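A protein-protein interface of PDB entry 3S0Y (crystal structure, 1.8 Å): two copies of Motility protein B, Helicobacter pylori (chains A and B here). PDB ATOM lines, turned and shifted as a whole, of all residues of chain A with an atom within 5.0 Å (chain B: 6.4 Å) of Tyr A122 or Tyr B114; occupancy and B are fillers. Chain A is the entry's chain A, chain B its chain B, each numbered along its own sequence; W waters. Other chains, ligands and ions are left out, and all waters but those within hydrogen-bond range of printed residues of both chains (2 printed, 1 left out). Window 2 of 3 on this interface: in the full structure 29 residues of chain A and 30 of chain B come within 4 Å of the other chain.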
ATOM      1  N   ALA A 117      29.348  -1.899 -18.624  1.00  0.00           N
ATOM      2  CA  ALA A 117      28.173  -1.738 -17.782  1.00  0.00           C
ATOM      3  C   ALA A 117      26.950  -1.326 -18.590  1.00  0.00           C
ATOM      4  O   ALA A 117      25.844  -1.866 -18.377  1.00  0.00           O
ATOM      5  CB  ALA A 117      28.451  -0.724 -16.672  1.00  0.00           C
ATOM      6  N   ALA A 118      27.134  -0.411 -19.548  1.00  0.00           N
ATOM      7  CA  ALA A 118      26.005   0.014 -20.404  1.00  0.00           C
ATOM      8  C   ALA A 118      25.417  -1.167 -21.201  1.00  0.00           C
ATOM      9  O   ALA A 118      24.209  -1.327 -21.300  1.00  0.00           O
ATOM     10  CB  ALA A 118      26.434   1.112 -21.367  1.00  0.00           C
ATOM     11  N   ASN A 119      26.286  -1.959 -21.804  1.00  0.00           N
ATOM     12  CA  ASN A 119      25.845  -3.125 -22.584  1.00  0.00           C
ATOM     13  C   ASN A 119      25.157  -4.182 -21.752  1.00  0.00           C
ATOM     14  O   ASN A 119      24.133  -4.719 -22.159  1.00  0.00           O
ATOM     15  CB  ASN A 119      27.023  -3.716 -23.330  1.00  0.00           C
ATOM     16  CG  ASN A 119      27.283  -2.996 -24.652  1.00  0.00           C
ATOM     17  OD1 ASN A 119      26.738  -3.391 -25.674  1.00  0.00           O
ATOM     18  ND2 ASN A 119      28.138  -1.964 -24.640  1.00  0.00           N
ATOM     19  N   ARG A 120      25.666  -4.427 -20.554  1.00  0.00           N
ATOM     20  CA  ARG A 120      25.012  -5.341 -19.643  1.00  0.00           C
ATOM     21  C   ARG A 120      23.590  -4.902 -19.259  1.00  0.00           C
ATOM     22  O   ARG A 120      22.646  -5.683 -19.366  1.00  0.00           O
ATOM     23  CB  ARG A 120      25.901  -5.575 -18.434  1.00  0.00           C
ATOM     24  CG  ARG A 120      27.079  -6.464 -18.786  1.00  0.00           C
ATOM     25  CD  ARG A 120      28.139  -6.421 -17.740  1.00  0.00           C
ATOM     26  NE  ARG A 120      27.762  -7.029 -16.471  1.00  0.00           N
ATOM     27  CZ  ARG A 120      27.976  -8.293 -16.121  1.00  0.00           C
ATOM     28  NH1 ARG A 120      28.496  -9.166 -16.978  1.00  0.00           N
ATOM     29  NH2 ARG A 120      27.673  -8.687 -14.890  1.00  0.00           N
ATOM     30  N   ALA A 121      23.431  -3.635 -18.908  1.00  0.00           N
ATOM     31  CA  ALA A 121      22.137  -3.097 -18.531  1.00  0.00           C
ATOM     32  C   ALA A 121      21.167  -3.078 -19.728  1.00  0.00           C
ATOM     33  O   ALA A 121      20.002  -3.469 -19.621  1.00  0.00           O
ATOM     34  CB  ALA A 121      22.331  -1.678 -17.923  1.00  0.00           C
ATOM     35  N   TYR A 122      21.678  -2.671 -20.896  1.00  0.00           N
ATOM     36  CA  TYR A 122      20.916  -2.705 -22.130  1.00  0.00           C
ATOM     37  C   TYR A 122      20.394  -4.106 -22.443  1.00  0.00           C
ATOM     38  O   TYR A 122      19.218  -4.284 -22.773  1.00  0.00           O
ATOM     39  CB  TYR A 122      21.824  -2.229 -23.286  1.00  0.00           C
ATOM     40  CG  TYR A 122      21.216  -2.381 -24.643  1.00  0.00           C
ATOM     41  CD1 TYR A 122      20.263  -1.485 -25.095  1.00  0.00           C
ATOM     42  CD2 TYR A 122      21.593  -3.430 -25.484  1.00  0.00           C
ATOM     43  CE1 TYR A 122      19.727  -1.596 -26.375  1.00  0.00           C
ATOM     44  CE2 TYR A 122      21.050  -3.566 -26.742  1.00  0.00           C
ATOM     45  CZ  TYR A 122      20.113  -2.646 -27.185  1.00  0.00           C
ATOM     46  OH  TYR A 122      19.577  -2.792 -28.437  1.00  0.00           O
ATOM     47  N   ARG A 123      21.264  -5.111 -22.357  1.00  0.00           N
ATOM     48  CA  ARG A 123      20.853  -6.461 -22.697  1.00  0.00           C
ATOM     49  C   ARG A 123      19.736  -6.905 -21.760  1.00  0.00           C
ATOM     50  O   ARG A 123      18.739  -7.443 -22.232  1.00  0.00           O
ATOM     51  CB  ARG A 123      22.029  -7.432 -22.651  1.00  0.00           C
ATOM     52  CG  ARG A 123      21.753  -8.851 -23.212  1.00  0.00           C
ATOM     53  CD  ARG A 123      20.950  -8.923 -24.532  1.00  0.00           C
ATOM     54  NE  ARG A 123      21.508  -8.167 -25.673  1.00  0.00           N
ATOM     55  CZ  ARG A 123      20.811  -7.745 -26.731  1.00  0.00           C
ATOM     56  NH1 ARG A 123      19.504  -7.974 -26.832  1.00  0.00           N
ATOM     57  NH2 ARG A 123      21.412  -7.070 -27.707  1.00  0.00           N
ATOM     58  N   VAL A 124      19.880  -6.665 -20.461  1.00  0.00           N
ATOM     59  CA  VAL A 124      18.825  -7.049 -19.495  1.00  0.00           C
ATOM     60  C   VAL A 124      17.480  -6.361 -19.833  1.00  0.00           C
ATOM     61  O   VAL A 124      16.426  -7.002 -19.835  1.00  0.00           O
ATOM     62  CB  VAL A 124      19.195  -6.787 -18.025  1.00  0.00           C
ATOM     63  CG1 VAL A 124      17.949  -6.961 -17.076  1.00  0.00           C
ATOM     64  CG2 VAL A 124      20.370  -7.710 -17.598  1.00  0.00           C
ATOM     65  N   MET A 125      17.538  -5.067 -20.098  1.00  0.00           N
ATOM     66  CA  MET A 125      16.386  -4.297 -20.545  1.00  0.00           C
ATOM     67  C   MET A 125      15.726  -4.934 -21.759  1.00  0.00           C
ATOM     68  O   MET A 125      14.500  -5.099 -21.772  1.00  0.00           O
ATOM     69  CB  MET A 125      16.783  -2.840 -20.851  1.00  0.00           C
ATOM     70  CG  MET A 125      15.590  -1.891 -21.067  1.00  0.00           C
ATOM     71  SD  MET A 125      16.122  -0.332 -21.831  1.00  0.00           S
ATOM     72  CE  MET A 125      16.578  -0.916 -23.446  1.00  0.00           C
ATOM     73  N   LYS A 126      16.521  -5.320 -22.751  1.00  0.00           N
ATOM     74  CA  LYS A 126      15.973  -5.889 -23.977  1.00  0.00           C
ATOM     75  C   LYS A 126      15.291  -7.223 -23.689  1.00  0.00           C
ATOM     76  O   LYS A 126      14.242  -7.509 -24.273  1.00  0.00           O
ATOM     77  CB  LYS A 126      17.020  -5.986 -25.068  1.00  0.00           C
ATOM     78  CG  LYS A 126      17.502  -4.594 -25.538  1.00  0.00           C
ATOM     79  CD  LYS A 126      16.523  -3.934 -26.523  1.00  0.00           C
ATOM     80  CE  LYS A 126      16.699  -4.522 -27.930  1.00  0.00           C
ATOM     81  NZ  LYS A 126      15.766  -3.916 -28.924  1.00  0.00           N
ATOM     82  N   ILE A 129      11.968  -6.639 -22.264  1.00  0.00           N
ATOM     83  CA  ILE A 129      11.072  -6.271 -23.357  1.00  0.00           C
ATOM     84  C   ILE A 129      10.605  -7.527 -24.099  1.00  0.00           C
ATOM     85  O   ILE A 129       9.427  -7.673 -24.417  1.00  0.00           O
ATOM     86  CB  ILE A 129      11.717  -5.243 -24.295  1.00  0.00           C
ATOM     87  CG1 ILE A 129      11.859  -3.928 -23.541  1.00  0.00           C
ATOM     88  CG2 ILE A 129      10.840  -5.058 -25.572  1.00  0.00           C
ATOM     89  CD1 ILE A 129      12.735  -2.908 -24.199  1.00  0.00           C
ATOM     90  N   PRO A 135       8.465  -0.984 -23.437  1.00  0.00           N
ATOM     91  CA  PRO A 135       9.679  -0.152 -23.523  1.00  0.00           C
ATOM     92  C   PRO A 135       9.491   1.267 -22.971  1.00  0.00           C
ATOM     93  O   PRO A 135      10.459   1.872 -22.489  1.00  0.00           O
ATOM     94  CB  PRO A 135       9.985  -0.117 -25.020  1.00  0.00           C
ATOM     95  CG  PRO A 135       9.228  -1.217 -25.627  1.00  0.00           C
ATOM     96  CD  PRO A 135       8.097  -1.550 -24.747  1.00  0.00           C
ATOM     97  N   PHE A 140      17.995   2.146 -19.367  1.00  0.00           N
ATOM     98  CA  PHE A 140      19.203   1.518 -18.841  1.00  0.00           C
ATOM     99  C   PHE A 140      20.265   2.576 -18.519  1.00  0.00           C
ATOM    100  O   PHE A 140      20.316   3.668 -19.146  1.00  0.00           O
ATOM    101  CB  PHE A 140      19.728   0.425 -19.792  1.00  0.00           C
ATOM    102  CG  PHE A 140      20.301   0.942 -21.108  1.00  0.00           C
ATOM    103  CD1 PHE A 140      21.676   1.114 -21.255  1.00  0.00           C
ATOM    104  CD2 PHE A 140      19.479   1.254 -22.183  1.00  0.00           C
ATOM    105  CE1 PHE A 140      22.218   1.596 -22.452  1.00  0.00           C
ATOM    106  CE2 PHE A 140      20.030   1.738 -23.402  1.00  0.00           C
ATOM    107  CZ  PHE A 140      21.398   1.904 -23.520  1.00  0.00           C
ATOM    108  N   THR B 100      16.073  10.480 -27.668  1.00  0.00           N
ATOM    109  CA  THR B 100      16.011  10.836 -29.103  1.00  0.00           C
ATOM    110  C   THR B 100      14.567  10.998 -29.555  1.00  0.00           C
ATOM    111  O   THR B 100      13.667  10.549 -28.892  1.00  0.00           O
ATOM    112  CB  THR B 100      16.669   9.768 -30.005  1.00  0.00           C
ATOM    113  OG1 THR B 100      15.891   8.574 -29.973  1.00  0.00           O
ATOM    114  CG2 THR B 100      18.123   9.457 -29.609  1.00  0.00           C
ATOM    115  N   SER B 112      21.192   2.369 -33.309  1.00  0.00           N
ATOM    116  CA  SER B 112      19.915   2.394 -32.608  1.00  0.00           C
ATOM    117  C   SER B 112      19.735   3.749 -31.924  1.00  0.00           C
ATOM    118  O   SER B 112      20.726   4.454 -31.662  1.00  0.00           O
ATOM    119  CB  SER B 112      19.835   1.271 -31.562  1.00  0.00           C
ATOM    120  OG  SER B 112      20.714   1.494 -30.447  1.00  0.00           O
ATOM    121  N   HIS B 113      18.489   4.117 -31.642  1.00  0.00           N
ATOM    122  CA  HIS B 113      18.226   5.297 -30.818  1.00  0.00           C
ATOM    123  C   HIS B 113      18.780   5.127 -29.396  1.00  0.00           C
ATOM    124  O   HIS B 113      19.250   6.099 -28.804  1.00  0.00           O
ATOM    125  CB  HIS B 113      16.734   5.635 -30.743  1.00  0.00           C
ATOM    126  CG  HIS B 113      16.150   6.065 -32.059  1.00  0.00           C
ATOM    127  ND1 HIS B 113      15.286   5.278 -32.780  1.00  0.00           N
ATOM    128  CD2 HIS B 113      16.333   7.189 -32.790  1.00  0.00           C
ATOM    129  CE1 HIS B 113      14.949   5.901 -33.899  1.00  0.00           C
ATOM    130  NE2 HIS B 113      15.568   7.065 -33.926  1.00  0.00           N
ATOM    131  N   TYR B 114      18.712   3.911 -28.856  1.00  0.00           N
ATOM    132  CA  TYR B 114      19.291   3.643 -27.521  1.00  0.00           C
ATOM    133  C   TYR B 114      20.779   3.956 -27.530  1.00  0.00           C
ATOM    134  O   TYR B 114      21.286   4.622 -26.610  1.00  0.00           O
ATOM    135  CB  TYR B 114      19.070   2.198 -27.086  1.00  0.00           C
ATOM    136  CG  TYR B 114      17.660   1.857 -26.661  1.00  0.00           C
ATOM    137  CD1 TYR B 114      17.043   2.504 -25.590  1.00  0.00           C
ATOM    138  CD2 TYR B 114      16.965   0.855 -27.302  1.00  0.00           C
ATOM    139  CE1 TYR B 114      15.743   2.155 -25.221  1.00  0.00           C
ATOM    140  CE2 TYR B 114      15.710   0.508 -26.930  1.00  0.00           C
ATOM    141  CZ  TYR B 114      15.100   1.166 -25.892  1.00  0.00           C
ATOM    142  OH  TYR B 114      13.814   0.777 -25.555  1.00  0.00           O
ATOM    143  N   GLU B 115      21.471   3.539 -28.583  1.00  0.00           N
ATOM    144  CA  GLU B 115      22.925   3.740 -28.657  1.00  0.00           C
ATOM    145  C   GLU B 115      23.268   5.204 -28.798  1.00  0.00           C
ATOM    146  O   GLU B 115      24.113   5.704 -28.078  1.00  0.00           O
ATOM    147  CB  GLU B 115      23.559   2.951 -29.796  1.00  0.00           C
ATOM    148  CG  GLU B 115      25.081   3.031 -29.819  1.00  0.00           C
ATOM    149  CD  GLU B 115      25.680   2.306 -31.019  1.00  0.00           C
ATOM    150  OE1 GLU B 115      25.205   2.540 -32.152  1.00  0.00           O
ATOM    151  OE2 GLU B 115      26.610   1.495 -30.843  1.00  0.00           O
ATOM    152  N   LEU B 116      22.623   5.890 -29.739  1.00  0.00           N
ATOM    153  CA  LEU B 116      22.851   7.325 -29.884  1.00  0.00           C
ATOM    154  C   LEU B 116      22.574   8.094 -28.577  1.00  0.00           C
ATOM    155  O   LEU B 116      23.378   8.937 -28.168  1.00  0.00           O
ATOM    156  CB  LEU B 116      22.014   7.876 -31.044  1.00  0.00           C
ATOM    157  CG  LEU B 116      21.989   9.393 -31.189  1.00  0.00           C
ATOM    158  CD1 LEU B 116      23.408   9.902 -31.459  1.00  0.00           C
ATOM    159  CD2 LEU B 116      20.983   9.794 -32.300  1.00  0.00           C
ATOM    160  N   ALA B 117      21.439   7.827 -27.940  1.00  0.00           N
ATOM    161  CA  ALA B 117      21.088   8.517 -26.696  1.00  0.00           C
ATOM    162  C   ALA B 117      22.141   8.234 -25.585  1.00  0.00           C
ATOM    163  O   ALA B 117      22.498   9.148 -24.828  1.00  0.00           O
ATOM    164  CB  ALA B 117      19.682   8.112 -26.232  1.00  0.00           C
ATOM    165  N   ALA B 118      22.627   6.998 -25.511  1.00  0.00           N
ATOM    166  CA  ALA B 118      23.653   6.609 -24.524  1.00  0.00           C
ATOM    167  C   ALA B 118      24.939   7.379 -24.771  1.00  0.00           C
ATOM    168  O   ALA B 118      25.540   7.909 -23.850  1.00  0.00           O
ATOM    169  CB  ALA B 118      23.914   5.105 -24.557  1.00  0.00           C
ATOM    170  N   ASN B 119      25.356   7.467 -26.030  1.00  0.00           N
ATOM    171  CA  ASN B 119      26.579   8.190 -26.346  1.00  0.00           C
ATOM    172  C   ASN B 119      26.501   9.678 -26.053  1.00  0.00           C
ATOM    173  O   ASN B 119      27.446  10.281 -25.546  1.00  0.00           O
ATOM    174  CB  ASN B 119      27.000   7.955 -27.804  1.00  0.00           C
ATOM    175  CG  ASN B 119      27.772   6.662 -27.962  1.00  0.00           C
ATOM    176  OD1 ASN B 119      28.988   6.660 -27.883  1.00  0.00           O
ATOM    177  ND2 ASN B 119      27.049   5.532 -28.126  1.00  0.00           N
ATOM    178  N   SER B 142      20.170   5.935 -20.959  1.00  0.00           N
ATOM    179  CA  SER B 142      19.540   6.080 -22.253  1.00  0.00           C
ATOM    180  C   SER B 142      18.101   5.618 -22.206  1.00  0.00           C
ATOM    181  O   SER B 142      17.797   4.538 -21.683  1.00  0.00           O
ATOM    182  CB  SER B 142      20.288   5.232 -23.270  1.00  0.00           C
ATOM    183  OG  SER B 142      19.600   5.234 -24.502  1.00  0.00           O
ATOM    184  N   TYR B 143      17.220   6.459 -22.765  1.00  0.00           N
ATOM    185  CA  TYR B 143      15.811   6.136 -22.923  1.00  0.00           C
ATOM    186  C   TYR B 143      15.490   5.872 -24.413  1.00  0.00           C
ATOM    187  O   TYR B 143      14.356   5.576 -24.757  1.00  0.00           O
ATOM    188  CB  TYR B 143      14.969   7.297 -22.409  1.00  0.00           C
ATOM    189  CG  TYR B 143      15.043   7.506 -20.940  1.00  0.00           C
ATOM    190  CD1 TYR B 143      13.956   7.180 -20.137  1.00  0.00           C
ATOM    191  CD2 TYR B 143      16.212   7.953 -20.319  1.00  0.00           C
ATOM    192  CE1 TYR B 143      13.999   7.348 -18.775  1.00  0.00           C
ATOM    193  CE2 TYR B 143      16.265   8.112 -18.935  1.00  0.00           C
ATOM    194  CZ  TYR B 143      15.148   7.807 -18.174  1.00  0.00           C
ATOM    195  OH  TYR B 143      15.157   7.951 -16.811  1.00  0.00           O
ATOM    196  N   GLY B 144      16.474   6.002 -25.304  1.00  0.00           N
ATOM    197  CA  GLY B 144      16.234   5.850 -26.726  1.00  0.00           C
ATOM    198  C   GLY B 144      15.161   6.844 -27.129  1.00  0.00           C
ATOM    199  O   GLY B 144      15.201   8.005 -26.676  1.00  0.00           O
ATOM    200  N   SER B 145      14.192   6.379 -27.920  1.00  0.00           N
ATOM    201  CA  SER B 145      13.122   7.248 -28.420  1.00  0.00           C
ATOM    202  C   SER B 145      11.869   7.197 -27.524  1.00  0.00           C
ATOM    203  O   SER B 145      10.826   7.716 -27.893  1.00  0.00           O
ATOM    204  CB  SER B 145      12.767   6.836 -29.843  1.00  0.00           C
ATOM    205  OG  SER B 145      12.248   5.499 -29.865  1.00  0.00           O
ATOM    206  N   THR B 146      11.960   6.536 -26.373  1.00  0.00           N
ATOM    207  CA  THR B 146      10.833   6.451 -25.450  1.00  0.00           C
ATOM    208  C   THR B 146      10.746   7.726 -24.594  1.00  0.00           C
ATOM    209  O   THR B 146      11.654   8.548 -24.590  1.00  0.00           O
ATOM    210  CB  THR B 146      10.964   5.221 -24.523  1.00  0.00           C
ATOM    211  OG1 THR B 146      11.905   5.503 -23.490  1.00  0.00           O
ATOM    212  CG2 THR B 146      11.410   3.974 -25.314  1.00  0.00           C
HETATM  213  O   HOH W   1      13.076   1.598 -23.401  1.00  0.00           O
HETATM  214  O   HOH W   2      21.700  -0.769 -29.813  1.00  0.00           O
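O of Tyr B114 is in hydrogen-bond range of OG of Ser B142. O of Tyr B143 is in hydrogen-bond range of OG1 of Thr B146. The backbone NH (N) of Gly B144 is in hydrogen-bond range of the side-chain hydroxyl (OG) of Ser B142, at 3.3 Å.
Of the 14 printed residues of chain B, 3 touch a printed residue of chain A. Hydrophobic or aromatic side chains of chain B that line the printed part of chain A: Tyr B114. Hydrophobic or aromatic side chains of chain A that line the printed part of chain B: Tyr A122, Met A125, Pro A135 and Phe A140. Along chain A the printed residues that touch a printed residue of chain B span positions 122 to 140. Among the printed residues, no Asp or Glu carboxylate lies within 4 Å of a Lys or Arg side-chain nitrogen of the other chain.
The backbone carbonyl oxygen (O) of Phe A140 is in hydrogen-bond range of the backbone NH (N) of Ser B142 (2.9 Å).
Positions printed for both chains: 117, 118 and 119.
Water W1 bridges OH of Tyr B114 (2.4 Å) and O of Pro A135 (2.8 Å). Water W2 bridges OG of Ser B112 and OH of Tyr A122.
Among the printed residues, pairs that only touch across the chains: Met A125 with Tyr B114 (3.5 Å), Pro A135 with Thr B146 (3.6 Å), Phe A140 with Tyr B114 (3.8 Å), Tyr A122 with Tyr B114 (3.8 Å) and Pro A135 with Tyr B114 (3.97 Å).
Tyr B114 touches just these residues of chain A: Tyr A122 (3.8 Å), Met A125 (3.5 Å), Pro A135 (3.97 Å) and Phe A140 (3.8 Å). Of the printed residues of chain B, Pro A135 touches Tyr B114 (3.97 Å) and Thr B146 (3.6 Å). Printed residues of chain A within 4 Å of Ser B142: Phe A140 (2.9 Å). Of the printed residues of chain B, Phe A140 touches Tyr B114 and Ser B142. Lys A126 touches none of the printed residues of chain B. The nearest residue of chain A that does not touch Tyr B114 is Ile A129 (4.1 Å).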
